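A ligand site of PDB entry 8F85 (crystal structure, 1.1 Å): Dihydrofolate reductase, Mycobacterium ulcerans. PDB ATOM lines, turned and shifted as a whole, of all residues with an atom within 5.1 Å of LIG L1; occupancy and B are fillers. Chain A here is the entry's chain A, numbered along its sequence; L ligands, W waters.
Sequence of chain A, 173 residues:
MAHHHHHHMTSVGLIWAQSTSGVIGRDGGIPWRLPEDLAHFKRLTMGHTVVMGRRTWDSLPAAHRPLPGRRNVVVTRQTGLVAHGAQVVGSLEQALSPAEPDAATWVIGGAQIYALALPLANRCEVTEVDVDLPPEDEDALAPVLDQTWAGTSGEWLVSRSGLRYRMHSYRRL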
ATOM      1  N   ILE A  15     -27.742  16.512 -22.525  1.00  0.00           N
ATOM      2  CA  ILE A  15     -27.441  16.039 -23.874  1.00  0.00           C
ATOM      3  C   ILE A  15     -26.193  15.191 -23.777  1.00  0.00           C
ATOM      4  O   ILE A  15     -25.201  15.597 -23.155  1.00  0.00           O
ATOM      5  CB  ILE A  15     -27.290  17.232 -24.853  1.00  0.00           C
ATOM      6  CG1 ILE A  15     -27.034  16.742 -26.283  1.00  0.00           C
ATOM      7  CG2 ILE A  15     -26.244  18.259 -24.405  1.00  0.00           C
ATOM      8  CD1 ILE A  15     -27.258  17.808 -27.338  1.00  0.00           C
ATOM      9  N   TRP A  16     -26.253  13.983 -24.356  1.00  0.00           N
ATOM     10  CA  TRP A  16     -25.117  13.076 -24.348  1.00  0.00           C
ATOM     11  C   TRP A  16     -25.208  12.146 -25.546  1.00  0.00           C
ATOM     12  O   TRP A  16     -26.271  11.986 -26.148  1.00  0.00           O
ATOM     13  CB  TRP A  16     -24.997  12.251 -23.068  1.00  0.00           C
ATOM     14  CG  TRP A  16     -25.977  11.120 -22.846  1.00  0.00           C
ATOM     15  CD1 TRP A  16     -25.825   9.820 -23.226  1.00  0.00           C
ATOM     16  CD2 TRP A  16     -27.197  11.168 -22.088  1.00  0.00           C
ATOM     17  NE1 TRP A  16     -26.867   9.056 -22.759  1.00  0.00           N
ATOM     18  CE2 TRP A  16     -27.730   9.857 -22.075  1.00  0.00           C
ATOM     19  CE3 TRP A  16     -27.899  12.180 -21.437  1.00  0.00           C
ATOM     20  CZ2 TRP A  16     -28.908   9.547 -21.412  1.00  0.00           C
ATOM     21  CZ3 TRP A  16     -29.069  11.874 -20.786  1.00  0.00           C
ATOM     22  CH2 TRP A  16     -29.567  10.561 -20.777  1.00  0.00           C
ATOM     23  N   ALA A  17     -24.090  11.524 -25.846  1.00  0.00           N
ATOM     24  CA  ALA A  17     -24.004  10.417 -26.785  1.00  0.00           C
ATOM     25  C   ALA A  17     -23.434   9.208 -26.075  1.00  0.00           C
ATOM     26  O   ALA A  17     -22.506   9.321 -25.271  1.00  0.00           O
ATOM     27  CB  ALA A  17     -23.141  10.792 -27.981  1.00  0.00           C
ATOM     28  N   ILE A  24     -19.953   6.412 -22.321  1.00  0.00           N
ATOM     29  CA  ILE A  24     -19.842   7.779 -22.799  1.00  0.00           C
ATOM     30  C   ILE A  24     -18.411   8.294 -22.872  1.00  0.00           C
ATOM     31  O   ILE A  24     -18.154   9.256 -23.596  1.00  0.00           O
ATOM     32  CB  ILE A  24     -20.722   8.764 -21.993  1.00  0.00           C
ATOM     33  CG1 ILE A  24     -20.212   8.967 -20.554  1.00  0.00           C
ATOM     34  CG2 ILE A  24     -22.168   8.343 -22.051  1.00  0.00           C
ATOM     35  CD1 ILE A  24     -20.891  10.148 -19.869  1.00  0.00           C
ATOM     36  N   ILE A  30     -13.268  10.296 -25.925  1.00  0.00           N
ATOM     37  CA  ILE A  30     -14.432   9.645 -26.502  1.00  0.00           C
ATOM     38  C   ILE A  30     -13.949   8.478 -27.352  1.00  0.00           C
ATOM     39  O   ILE A  30     -13.153   8.686 -28.272  1.00  0.00           O
ATOM     40  CB  ILE A  30     -15.247  10.614 -27.378  1.00  0.00           C
ATOM     41  CG1 ILE A  30     -15.606  11.898 -26.621  1.00  0.00           C
ATOM     42  CG2 ILE A  30     -16.483   9.898 -27.929  1.00  0.00           C
ATOM     43  CD1 ILE A  30     -16.431  11.686 -25.384  1.00  0.00           C
ATOM     44  N   TRP A  32     -15.046   6.867 -29.903  1.00  0.00           N
ATOM     45  CA  TRP A  32     -15.564   6.774 -31.263  1.00  0.00           C
ATOM     46  C   TRP A  32     -15.431   8.163 -31.874  1.00  0.00           C
ATOM     47  O   TRP A  32     -15.148   9.150 -31.178  1.00  0.00           O
ATOM     48  CB  TRP A  32     -17.032   6.295 -31.305  1.00  0.00           C
ATOM     49  CG  TRP A  32     -17.965   7.262 -30.609  1.00  0.00           C
ATOM     50  CD1 TRP A  32     -18.437   8.449 -31.098  1.00  0.00           C
ATOM     51  CD2 TRP A  32     -18.522   7.122 -29.296  1.00  0.00           C
ATOM     52  NE1 TRP A  32     -19.236   9.060 -30.157  1.00  0.00           N
ATOM     53  CE2 TRP A  32     -19.308   8.268 -29.051  1.00  0.00           C
ATOM     54  CE3 TRP A  32     -18.414   6.152 -28.307  1.00  0.00           C
ATOM     55  CZ2 TRP A  32     -19.973   8.466 -27.837  1.00  0.00           C
ATOM     56  CZ3 TRP A  32     -19.079   6.346 -27.110  1.00  0.00           C
ATOM     57  CH2 TRP A  32     -19.856   7.485 -26.886  1.00  0.00           C
ATOM     58  N   ASP A  37     -23.032  13.499 -34.810  1.00  0.00           N
ATOM     59  CA  ASP A  37     -23.369  13.835 -33.436  1.00  0.00           C
ATOM     60  C   ASP A  37     -22.710  15.142 -33.007  1.00  0.00           C
ATOM     61  O   ASP A  37     -23.327  15.962 -32.339  1.00  0.00           O
ATOM     62  CB  ASP A  37     -22.972  12.719 -32.499  1.00  0.00           C
ATOM     63  CG  ASP A  37     -23.178  13.152 -31.085  1.00  0.00           C
ATOM     64  OD1 ASP A  37     -24.334  13.270 -30.667  1.00  0.00           O
ATOM     65  OD2 ASP A  37     -22.174  13.432 -30.391  1.00  0.00           O
ATOM     66  N   LEU A  38     -21.464  15.348 -33.400  1.00  0.00           N
ATOM     67  CA  LEU A  38     -20.821  16.628 -33.119  1.00  0.00           C
ATOM     68  C   LEU A  38     -21.649  17.770 -33.704  1.00  0.00           C
ATOM     69  O   LEU A  38     -21.868  18.793 -33.056  1.00  0.00           O
ATOM     70  CB  LEU A  38     -19.388  16.598 -33.629  1.00  0.00           C
ATOM     71  CG  LEU A  38     -18.562  17.861 -33.436  1.00  0.00           C
ATOM     72  CD1 LEU A  38     -17.078  17.557 -33.297  1.00  0.00           C
ATOM     73  CD2 LEU A  38     -18.760  18.840 -34.562  1.00  0.00           C
ATOM     74  N   HIS A  40     -24.952  17.747 -34.472  1.00  0.00           N
ATOM     75  CA  HIS A  40     -26.182  17.805 -33.676  1.00  0.00           C
ATOM     76  C   HIS A  40     -25.968  18.578 -32.389  1.00  0.00           C
ATOM     77  O   HIS A  40     -26.761  19.458 -32.023  1.00  0.00           O
ATOM     78  CB  HIS A  40     -26.569  16.345 -33.416  1.00  0.00           C
ATOM     79  CG  HIS A  40     -27.650  16.113 -32.411  1.00  0.00           C
ATOM     80  ND1 HIS A  40     -28.982  16.362 -32.656  1.00  0.00           N
ATOM     81  CD2 HIS A  40     -27.591  15.525 -31.190  1.00  0.00           C
ATOM     82  CE1 HIS A  40     -29.696  15.967 -31.602  1.00  0.00           C
ATOM     83  NE2 HIS A  40     -28.869  15.449 -30.712  1.00  0.00           N
ATOM     84  N   PHE A  41     -24.887  18.253 -31.683  1.00  0.00           N
ATOM     85  CA  PHE A  41     -24.569  18.933 -30.438  1.00  0.00           C
ATOM     86  C   PHE A  41     -24.358  20.424 -30.653  1.00  0.00           C
ATOM     87  O   PHE A  41     -24.884  21.249 -29.905  1.00  0.00           O
ATOM     88  CB  PHE A  41     -23.305  18.271 -29.847  1.00  0.00           C
ATOM     89  CG  PHE A  41     -22.816  18.957 -28.625  1.00  0.00           C
ATOM     90  CD1 PHE A  41     -23.435  18.745 -27.390  1.00  0.00           C
ATOM     91  CD2 PHE A  41     -21.763  19.845 -28.698  1.00  0.00           C
ATOM     92  CE1 PHE A  41     -22.993  19.428 -26.264  1.00  0.00           C
ATOM     93  CE2 PHE A  41     -21.320  20.521 -27.564  1.00  0.00           C
ATOM     94  CZ  PHE A  41     -21.932  20.316 -26.366  1.00  0.00           C
ATOM     95  N   LYS A  42     -23.561  20.776 -31.659  1.00  0.00           N
ATOM     96  CA  LYS A  42     -23.266  22.173 -31.929  1.00  0.00           C
ATOM     97  C   LYS A  42     -24.539  22.921 -32.313  1.00  0.00           C
ATOM     98  O   LYS A  42     -24.750  24.047 -31.873  1.00  0.00           O
ATOM     99  CB  LYS A  42     -22.180  22.255 -33.024  1.00  0.00           C
ATOM    100  CG  LYS A  42     -21.289  23.495 -33.065  1.00  0.00           C
ATOM    101  CD  LYS A  42     -20.366  23.481 -34.319  1.00  0.00           C
ATOM    102  CE  LYS A  42     -19.306  22.369 -34.335  1.00  0.00           C
ATOM    103  NZ  LYS A  42     -18.545  22.228 -35.655  1.00  0.00           N
ATOM    104  N   THR A  45     -26.818  23.410 -29.107  1.00  0.00           N
ATOM    105  CA  THR A  45     -26.302  24.198 -27.997  1.00  0.00           C
ATOM    106  C   THR A  45     -25.878  25.612 -28.388  1.00  0.00           C
ATOM    107  O   THR A  45     -25.718  26.444 -27.497  1.00  0.00           O
ATOM    108  CB  THR A  45     -25.120  23.488 -27.307  1.00  0.00           C
ATOM    109  OG1 THR A  45     -24.044  23.306 -28.222  1.00  0.00           O
ATOM    110  CG2 THR A  45     -25.561  22.171 -26.671  1.00  0.00           C
ATOM    111  N   THR A  56     -14.817  16.970 -17.919  1.00  0.00           N
ATOM    112  CA  THR A  56     -15.253  17.224 -19.287  1.00  0.00           C
ATOM    113  C   THR A  56     -14.593  18.479 -19.849  1.00  0.00           C
ATOM    114  O   THR A  56     -14.146  18.500 -21.002  1.00  0.00           O
ATOM    115  CB  THR A  56     -16.782  17.287 -19.347  1.00  0.00           C
ATOM    116  OG1 THR A  56     -17.308  15.981 -19.094  1.00  0.00           O
ATOM    117  CG2 THR A  56     -17.284  17.729 -20.696  1.00  0.00           C
ATOM    118  N   LEU A  60     -11.941  18.668 -23.437  1.00  0.00           N
ATOM    119  CA  LEU A  60     -12.274  19.360 -24.673  1.00  0.00           C
ATOM    120  C   LEU A  60     -11.026  19.586 -25.505  1.00  0.00           C
ATOM    121  O   LEU A  60     -10.028  20.083 -24.977  1.00  0.00           O
ATOM    122  CB  LEU A  60     -12.934  20.701 -24.377  1.00  0.00           C
ATOM    123  CG  LEU A  60     -14.300  20.617 -23.719  1.00  0.00           C
ATOM    124  CD1 LEU A  60     -14.740  22.003 -23.315  1.00  0.00           C
ATOM    125  CD2 LEU A  60     -15.303  20.005 -24.661  1.00  0.00           C
ATOM    126  N   PRO A  61     -11.052  19.283 -26.802  1.00  0.00           N
ATOM    127  CA  PRO A  61      -9.892  19.601 -27.649  1.00  0.00           C
ATOM    128  C   PRO A  61      -9.676  21.094 -27.753  1.00  0.00           C
ATOM    129  O   PRO A  61     -10.580  21.909 -27.550  1.00  0.00           O
ATOM    130  CB  PRO A  61     -10.274  19.008 -29.013  1.00  0.00           C
ATOM    131  CG  PRO A  61     -11.368  18.065 -28.768  1.00  0.00           C
ATOM    132  CD  PRO A  61     -12.094  18.543 -27.545  1.00  0.00           C
ATOM    133  N   HIS A  64     -11.952  23.715 -29.076  1.00  0.00           N
ATOM    134  CA  HIS A  64     -13.273  23.615 -28.477  1.00  0.00           C
ATOM    135  C   HIS A  64     -13.244  23.911 -26.979  1.00  0.00           C
ATOM    136  O   HIS A  64     -14.207  23.589 -26.292  1.00  0.00           O
ATOM    137  CB  HIS A  64     -13.870  22.242 -28.767  1.00  0.00           C
ATOM    138  CG  HIS A  64     -13.941  21.941 -30.226  1.00  0.00           C
ATOM    139  ND1 HIS A  64     -15.062  22.198 -30.980  1.00  0.00           N
ATOM    140  CD2 HIS A  64     -13.006  21.487 -31.084  1.00  0.00           C
ATOM    141  CE1 HIS A  64     -14.829  21.866 -32.230  1.00  0.00           C
ATOM    142  NE2 HIS A  64     -13.582  21.440 -32.326  1.00  0.00           N
ATOM    143  N   LEU A  67     -16.024  26.066 -25.631  1.00  0.00           N
ATOM    144  CA  LEU A  67     -16.896  25.779 -26.758  1.00  0.00           C
ATOM    145  C   LEU A  67     -17.332  27.104 -27.354  1.00  0.00           C
ATOM    146  O   LEU A  67     -18.014  27.879 -26.669  1.00  0.00           O
ATOM    147  CB  LEU A  67     -18.091  24.980 -26.256  1.00  0.00           C
ATOM    148  CG  LEU A  67     -17.733  23.559 -25.786  1.00  0.00           C
ATOM    149  CD1 LEU A  67     -18.828  22.985 -24.899  1.00  0.00           C
ATOM    150  CD2 LEU A  67     -17.479  22.653 -26.949  1.00  0.00           C
ATOM    151  N   PRO A  68     -16.994  27.408 -28.602  1.00  0.00           N
ATOM    152  CA  PRO A  68     -17.278  28.757 -29.119  1.00  0.00           C
ATOM    153  C   PRO A  68     -18.756  29.016 -29.273  1.00  0.00           C
ATOM    154  O   PRO A  68     -19.529  28.136 -29.659  1.00  0.00           O
ATOM    155  CB  PRO A  68     -16.562  28.770 -30.483  1.00  0.00           C
ATOM    156  CG  PRO A  68     -15.476  27.773 -30.348  1.00  0.00           C
ATOM    157  CD  PRO A  68     -16.063  26.686 -29.480  1.00  0.00           C
ATOM    158  N   ARG A  70     -21.025  29.685 -27.018  1.00  0.00           N
ATOM    159  CA  ARG A  70     -21.829  29.196 -25.921  1.00  0.00           C
ATOM    160  C   ARG A  70     -21.260  29.730 -24.643  1.00  0.00           C
ATOM    161  O   ARG A  70     -20.070  30.004 -24.551  1.00  0.00           O
ATOM    162  CB  ARG A  70     -21.788  27.712 -25.913  1.00  0.00           C
ATOM    163  CG  ARG A  70     -22.748  27.258 -26.972  1.00  0.00           C
ATOM    164  CD  ARG A  70     -22.351  25.991 -27.659  1.00  0.00           C
ATOM    165  NE  ARG A  70     -21.151  26.075 -28.484  1.00  0.00           N
ATOM    166  CZ  ARG A  70     -20.608  25.000 -29.043  1.00  0.00           C
ATOM    167  NH1 ARG A  70     -21.137  23.801 -28.868  1.00  0.00           N
ATOM    168  NH2 ARG A  70     -19.480  25.121 -29.742  1.00  0.00           N
ATOM    169  N   ILE A 108     -23.884  19.078 -20.320  1.00  0.00           N
ATOM    170  CA  ILE A 108     -23.179  18.444 -21.414  1.00  0.00           C
ATOM    171  C   ILE A 108     -22.188  17.404 -20.952  1.00  0.00           C
ATOM    172  O   ILE A 108     -21.405  16.901 -21.761  1.00  0.00           O
ATOM    173  CB  ILE A 108     -22.526  19.473 -22.356  1.00  0.00           C
ATOM    174  CG1 ILE A 108     -21.335  20.184 -21.682  1.00  0.00           C
ATOM    175  CG2 ILE A 108     -23.547  20.473 -22.853  1.00  0.00           C
ATOM    176  CD1 ILE A 108     -20.395  20.826 -22.672  1.00  0.00           C
ATOM    177  N   GLY A 109     -22.228  17.043 -19.673  1.00  0.00           N
ATOM    178  CA  GLY A 109     -21.473  15.925 -19.143  1.00  0.00           C
ATOM    179  C   GLY A 109     -20.525  16.360 -18.046  1.00  0.00           C
ATOM    180  O   GLY A 109     -20.432  17.530 -17.699  1.00  0.00           O
ATOM    181  N   TYR A 114     -23.963  14.438 -14.923  1.00  0.00           N
ATOM    182  CA  TYR A 114     -25.280  13.973 -15.366  1.00  0.00           C
ATOM    183  C   TYR A 114     -26.076  13.398 -14.200  1.00  0.00           C
ATOM    184  O   TYR A 114     -27.289  13.594 -14.117  1.00  0.00           O
ATOM    185  CB  TYR A 114     -25.187  12.907 -16.459  1.00  0.00           C
ATOM    186  CG  TYR A 114     -24.705  13.339 -17.819  1.00  0.00           C
ATOM    187  CD1 TYR A 114     -25.190  14.479 -18.435  1.00  0.00           C
ATOM    188  CD2 TYR A 114     -23.795  12.573 -18.502  1.00  0.00           C
ATOM    189  CE1 TYR A 114     -24.753  14.847 -19.685  1.00  0.00           C
ATOM    190  CE2 TYR A 114     -23.355  12.918 -19.747  1.00  0.00           C
ATOM    191  CZ  TYR A 114     -23.835  14.067 -20.341  1.00  0.00           C
ATOM    192  OH  TYR A 114     -23.327  14.433 -21.558  1.00  0.00           O
ATOM    193  N   GLU A 125     -31.566  14.779 -24.533  1.00  0.00           N
ATOM    194  CA  GLU A 125     -31.327  14.556 -25.956  1.00  0.00           C
ATOM    195  C   GLU A 125     -30.167  13.584 -26.040  1.00  0.00           C
ATOM    196  O   GLU A 125     -29.033  13.922 -25.675  1.00  0.00           O
ATOM    197  CB  GLU A 125     -31.038  15.857 -26.678  1.00  0.00           C
ATOM    198  CG  GLU A 125     -32.214  16.813 -26.733  1.00  0.00           C
ATOM    199  CD  GLU A 125     -33.398  16.255 -27.511  1.00  0.00           C
ATOM    200  OE1 GLU A 125     -33.201  15.423 -28.432  1.00  0.00           O
ATOM    201  OE2 GLU A 125     -34.528  16.663 -27.206  1.00  0.00           O
ATOM    202  N   THR A 127     -27.887  10.689 -28.177  1.00  0.00           N
ATOM    203  CA  THR A 127     -27.444   9.998 -29.372  1.00  0.00           C
ATOM    204  C   THR A 127     -26.981   8.608 -28.992  1.00  0.00           C
ATOM    205  O   THR A 127     -26.152   8.453 -28.088  1.00  0.00           O
ATOM    206  CB  THR A 127     -26.315  10.737 -30.078  1.00  0.00           C
ATOM    207  OG1 THR A 127     -26.760  12.069 -30.334  1.00  0.00           O
ATOM    208  CG2 THR A 127     -25.926  10.051 -31.388  1.00  0.00           C
HETATM  209  C1  LIG L   1     -18.392  21.786 -30.316  1.00  0.00           C
HETATM  210  C2  LIG L   1     -15.556  16.763 -27.856  1.00  0.00           C
HETATM  211  C3  LIG L   1     -14.691  16.521 -28.894  1.00  0.00           C
HETATM  212  C4  LIG L   1     -17.767  20.393 -30.410  1.00  0.00           C
HETATM  213  C5  LIG L   1     -17.325  19.907 -29.055  1.00  0.00           C
HETATM  214  C6  LIG L   1     -16.406  18.717 -29.021  1.00  0.00           C
HETATM  215  C7  LIG L   1     -15.509  18.441 -30.039  1.00  0.00           C
HETATM  216  C8  LIG L   1     -14.659  17.348 -29.991  1.00  0.00           C
HETATM  217  C9  LIG L   1     -18.523  17.788 -24.925  1.00  0.00           C
HETATM  218  C10 LIG L   1     -21.305  15.826 -26.270  1.00  0.00           C
HETATM  219  C11 LIG L   1     -19.883  17.615 -25.556  1.00  0.00           C
HETATM  220  N1  LIG L   1     -23.670  15.400 -26.241  1.00  0.00           N
HETATM  221  C12 LIG L   1     -23.549  14.989 -27.516  1.00  0.00           C
HETATM  222  C13 LIG L   1     -17.789  15.295 -30.064  1.00  0.00           C
HETATM  223  C14 LIG L   1     -18.051  14.228 -29.232  1.00  0.00           C
HETATM  224  C15 LIG L   1     -19.418  13.101 -27.464  1.00  0.00           C
HETATM  225  C16 LIG L   1     -19.171  14.252 -28.395  1.00  0.00           C
HETATM  226  C17 LIG L   1     -18.620  16.389 -30.058  1.00  0.00           C
HETATM  227  C18 LIG L   1     -21.251  15.393 -27.574  1.00  0.00           C
HETATM  228  C19 LIG L   1     -20.023  15.352 -28.409  1.00  0.00           C
HETATM  229  C20 LIG L   1     -22.558  15.812 -25.638  1.00  0.00           C
HETATM  230  C21 LIG L   1     -19.719  16.424 -29.240  1.00  0.00           C
HETATM  231  C22 LIG L   1     -17.423  17.263 -25.809  1.00  0.00           C
HETATM  232  C23 LIG L   1     -16.419  17.845 -27.914  1.00  0.00           C
HETATM  233  F1  LIG L   1     -18.744  12.014 -27.796  1.00  0.00           F
HETATM  234  F2  LIG L   1     -19.058  13.420 -26.207  1.00  0.00           F
HETATM  235  F3  LIG L   1     -20.697  12.759 -27.405  1.00  0.00           F
HETATM  236  N2  LIG L   1     -24.652  14.566 -28.158  1.00  0.00           N
HETATM  237  N3  LIG L   1     -22.686  16.214 -24.344  1.00  0.00           N
HETATM  238  N4  LIG L   1     -22.390  14.968 -28.187  1.00  0.00           N
HETATM  239  O1  LIG L   1     -20.169  16.207 -25.601  1.00  0.00           O
HETATM  240  O2  LIG L   1     -17.311  18.144 -26.931  1.00  0.00           O
HETATM  241  O3  LIG L   1     -19.609  21.853 -30.080  1.00  0.00           O
HETATM  242  O4  LIG L   1     -17.647  22.770 -30.451  1.00  0.00           O
HETATM  243  P1  LG2 L   2     -17.223  15.005 -15.145  1.00  0.00           P
HETATM  244  O1  LG2 L   2     -17.072  15.706 -16.442  1.00  0.00           O
HETATM  245  O2  LG2 L   2     -18.596  14.695 -14.632  1.00  0.00           O
HETATM  246  O3  LG2 L   2     -16.379  15.861 -14.109  1.00  0.00           O
HETATM  247  C1  LG2 L   2     -16.204  15.409 -12.756  1.00  0.00           C
HETATM  248  C2  LG2 L   2     -15.673  16.562 -11.950  1.00  0.00           C
HETATM  249  O4  LG2 L   2     -16.761  17.486 -11.683  1.00  0.00           O
HETATM  250  C3  LG2 L   2     -15.146  16.199 -10.568  1.00  0.00           C
HETATM  251  O5  LG2 L   2     -13.847  15.633 -10.665  1.00  0.00           O
HETATM  252  C4  LG2 L   2     -15.226  17.550  -9.882  1.00  0.00           C
HETATM  253  O6  LG2 L   2     -14.243  18.452 -10.337  1.00  0.00           O
HETATM  254  C5  LG2 L   2     -16.574  18.057 -10.406  1.00  0.00           C
HETATM  255  N1  LG2 L   2     -17.688  17.714  -9.546  1.00  0.00           N
HETATM  256  C6  LG2 L   2     -18.380  16.525  -9.458  1.00  0.00           C
HETATM  257  N2  LG2 L   2     -19.316  16.542  -8.546  1.00  0.00           N
HETATM  258  C7  LG2 L   2     -19.226  17.810  -7.995  1.00  0.00           C
HETATM  259  C8  LG2 L   2     -19.951  18.448  -6.979  1.00  0.00           C
HETATM  260  N3  LG2 L   2     -20.948  17.871  -6.310  1.00  0.00           N
HETATM  261  N4  LG2 L   2     -19.620  19.723  -6.677  1.00  0.00           N
HETATM  262  C9  LG2 L   2     -18.609  20.302  -7.346  1.00  0.00           C
HETATM  263  N5  LG2 L   2     -17.865  19.796  -8.321  1.00  0.00           N
HETATM  264  C10 LG2 L   2     -18.234  18.542  -8.599  1.00  0.00           C
HETATM  265  O7  LG2 L   2     -16.336  13.666 -15.155  1.00  0.00           O
HETATM  266  P2  LG2 L   2     -16.544  12.198 -15.762  1.00  0.00           P
HETATM  267  O8  LG2 L   2     -17.797  11.588 -15.227  1.00  0.00           O
HETATM  268  O9  LG2 L   2     -15.264  11.482 -15.542  1.00  0.00           O
HETATM  269  O10 LG2 L   2     -16.784  12.450 -17.315  1.00  0.00           O
HETATM  270  C11 LG2 L   2     -15.697  12.794 -18.200  1.00  0.00           C
HETATM  271  C12 LG2 L   2     -15.638  11.773 -19.304  1.00  0.00           C
HETATM  272  O11 LG2 L   2     -16.872  11.768 -20.049  1.00  0.00           O
HETATM  273  C13 LG2 L   2     -14.540  11.983 -20.345  1.00  0.00           C
HETATM  274  O12 LG2 L   2     -14.140  10.724 -20.887  1.00  0.00           O
HETATM  275  C14 LG2 L   2     -15.274  12.787 -21.427  1.00  0.00           C
HETATM  276  O13 LG2 L   2     -14.611  12.670 -22.674  1.00  0.00           O
HETATM  277  C15 LG2 L   2     -16.615  12.056 -21.415  1.00  0.00           C
HETATM  278  N6  LG2 L   2     -17.772  12.818 -21.920  1.00  0.00           N
HETATM  279  C16 LG2 L   2     -18.631  12.180 -22.774  1.00  0.00           C
HETATM  280  C17 LG2 L   2     -19.785  12.829 -23.193  1.00  0.00           C
HETATM  281  C18 LG2 L   2     -20.714  12.130 -24.127  1.00  0.00           C
HETATM  282  O14 LG2 L   2     -21.833  12.625 -24.350  1.00  0.00           O
HETATM  283  N7  LG2 L   2     -20.348  10.987 -24.681  1.00  0.00           N
HETATM  284  C19 LG2 L   2     -20.057  14.110 -22.738  1.00  0.00           C
HETATM  285  C20 LG2 L   2     -19.188  14.723 -21.867  1.00  0.00           C
HETATM  286  C21 LG2 L   2     -18.056  14.069 -21.436  1.00  0.00           C
HETATM  287  P3  LG2 L   2     -12.893  18.667  -9.485  1.00  0.00           P
HETATM  288  O15 LG2 L   2     -13.303  19.086  -8.096  1.00  0.00           O
HETATM  289  O16 LG2 L   2     -12.178  17.345  -9.518  1.00  0.00           O
HETATM  290  O17 LG2 L   2     -12.177  19.734 -10.273  1.00  0.00           O
HETATM  291  O   HOH W   1     -17.263  24.698 -33.047  1.00  0.00           O
HETATM  292  O   HOH W   2     -27.612  13.965 -28.329  1.00  0.00           O
HETATM  293  O   HOH W   3     -19.962  11.777 -30.938  1.00  0.00           O
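The guanidinium group (NE) of Arg 70 lies within hydrogen-bond range of the backbone carbonyl oxygen (O) of Pro 68. N of Trp 16 is in hydrogen-bond range of O of Glu 125, at 3.1 Å. The side-chain hydroxyl (OG1) of Thr 127 sits at hydrogen-bond distance from the side-chain carboxylate (OD1) of Asp 37. The side-chain hydroxyl of Thr 45 is in hydrogen-bond range of the backbone carbonyl oxygen of Phe 41, at 2.8 Å. The backbone carbonyl oxygen (O) of Ile 108 lies within hydrogen-bond range of the side-chain hydroxyl (OH) of Tyr 114 (3.1 Å). N of Gly 109 sits close to OH of Tyr 114 (3.4 Å). O of Trp 16 is in hydrogen-bond range of N of Thr 127 (2.9 Å). The guanidinium group (NH1) of Arg 70 sits at hydrogen-bond distance from the side-chain hydroxyl (OG1) of Thr 45 (3.0 Å).
The backbone NH (N) of Thr 56 sits at hydrogen-bond distance from an oxygen (O1) of LG2 L2, at 3.0 Å. NH1 of Arg 70 lies within salt-bridge range of O3 of LIG L1, at 2.8 Å. O of Ala 17 lies within hydrogen-bond range of N7 of LG2 L2. A nitrogen (N1) of LIG L1 sits close to the backbone NH (N) of Trp 16, 3.5 Å away. A nitrogen (N7) of LG2 L2 lies within hydrogen-bond range of the backbone carbonyl oxygen (O) of Ile 24. A nitrogen (N3) of LIG L1 lies within hydrogen-bond range of the backbone carbonyl oxygen of Ile 108 (3.0 Å). N4 of LIG L1 sits at hydrogen-bond distance from OD2 of Asp 37 (2.7 Å). N of Ala 17 sits at hydrogen-bond distance from O14 of LG2 L2 (2.9 Å). ND1 of His 64 sits at hydrogen-bond distance from O4 of LIG L1 (2.7 Å). OG1 of Thr 56 is in hydrogen-bond range of O1 of LG2 L2 (2.7 Å). The backbone carbonyl oxygen of Ile 15 lies within hydrogen-bond range of a nitrogen (N3) of LIG L1, at 2.8 Å. The side-chain hydroxyl (OH) of Tyr 114 is in hydrogen-bond range of a nitrogen (N3) of LIG L1 (3.4 Å).
Residues that only touch LIG L1: Ile 30, Ala 17, Phe 41, Leu 67, Leu 60, Pro 61, Leu 38, Trp 32, Lys 42 and Thr 127. Hydrophobic or aromatic side chains that line LIG L1: Ile 15, Ala 17, Ile 30, Trp 32, Leu 38, Phe 41, Leu 60, Pro 61, His 64, Leu 67 and Ile 108. 17 residues have an atom within 4 Å of LIG L1: Ile 15, Trp 16, Ala 17, Ile 30, Trp 32, Asp 37, Leu 38, Phe 41, Lys 42, Leu 60, Pro 61, His 64, Leu 67, Arg 70, Ile 108, Tyr 114 and Thr 127.
Water W2 lies within hydrogen-bond range of OG1 of Thr 127, O of Glu 125, N2 of LIG L1, NE2 of His 40 and O of Trp 16. Water W3 bridges the side-chain carboxylate (OD2) of Asp 37 (2.8 Å) and the indole nitrogen (NE1) of Trp 32 (2.9 Å).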
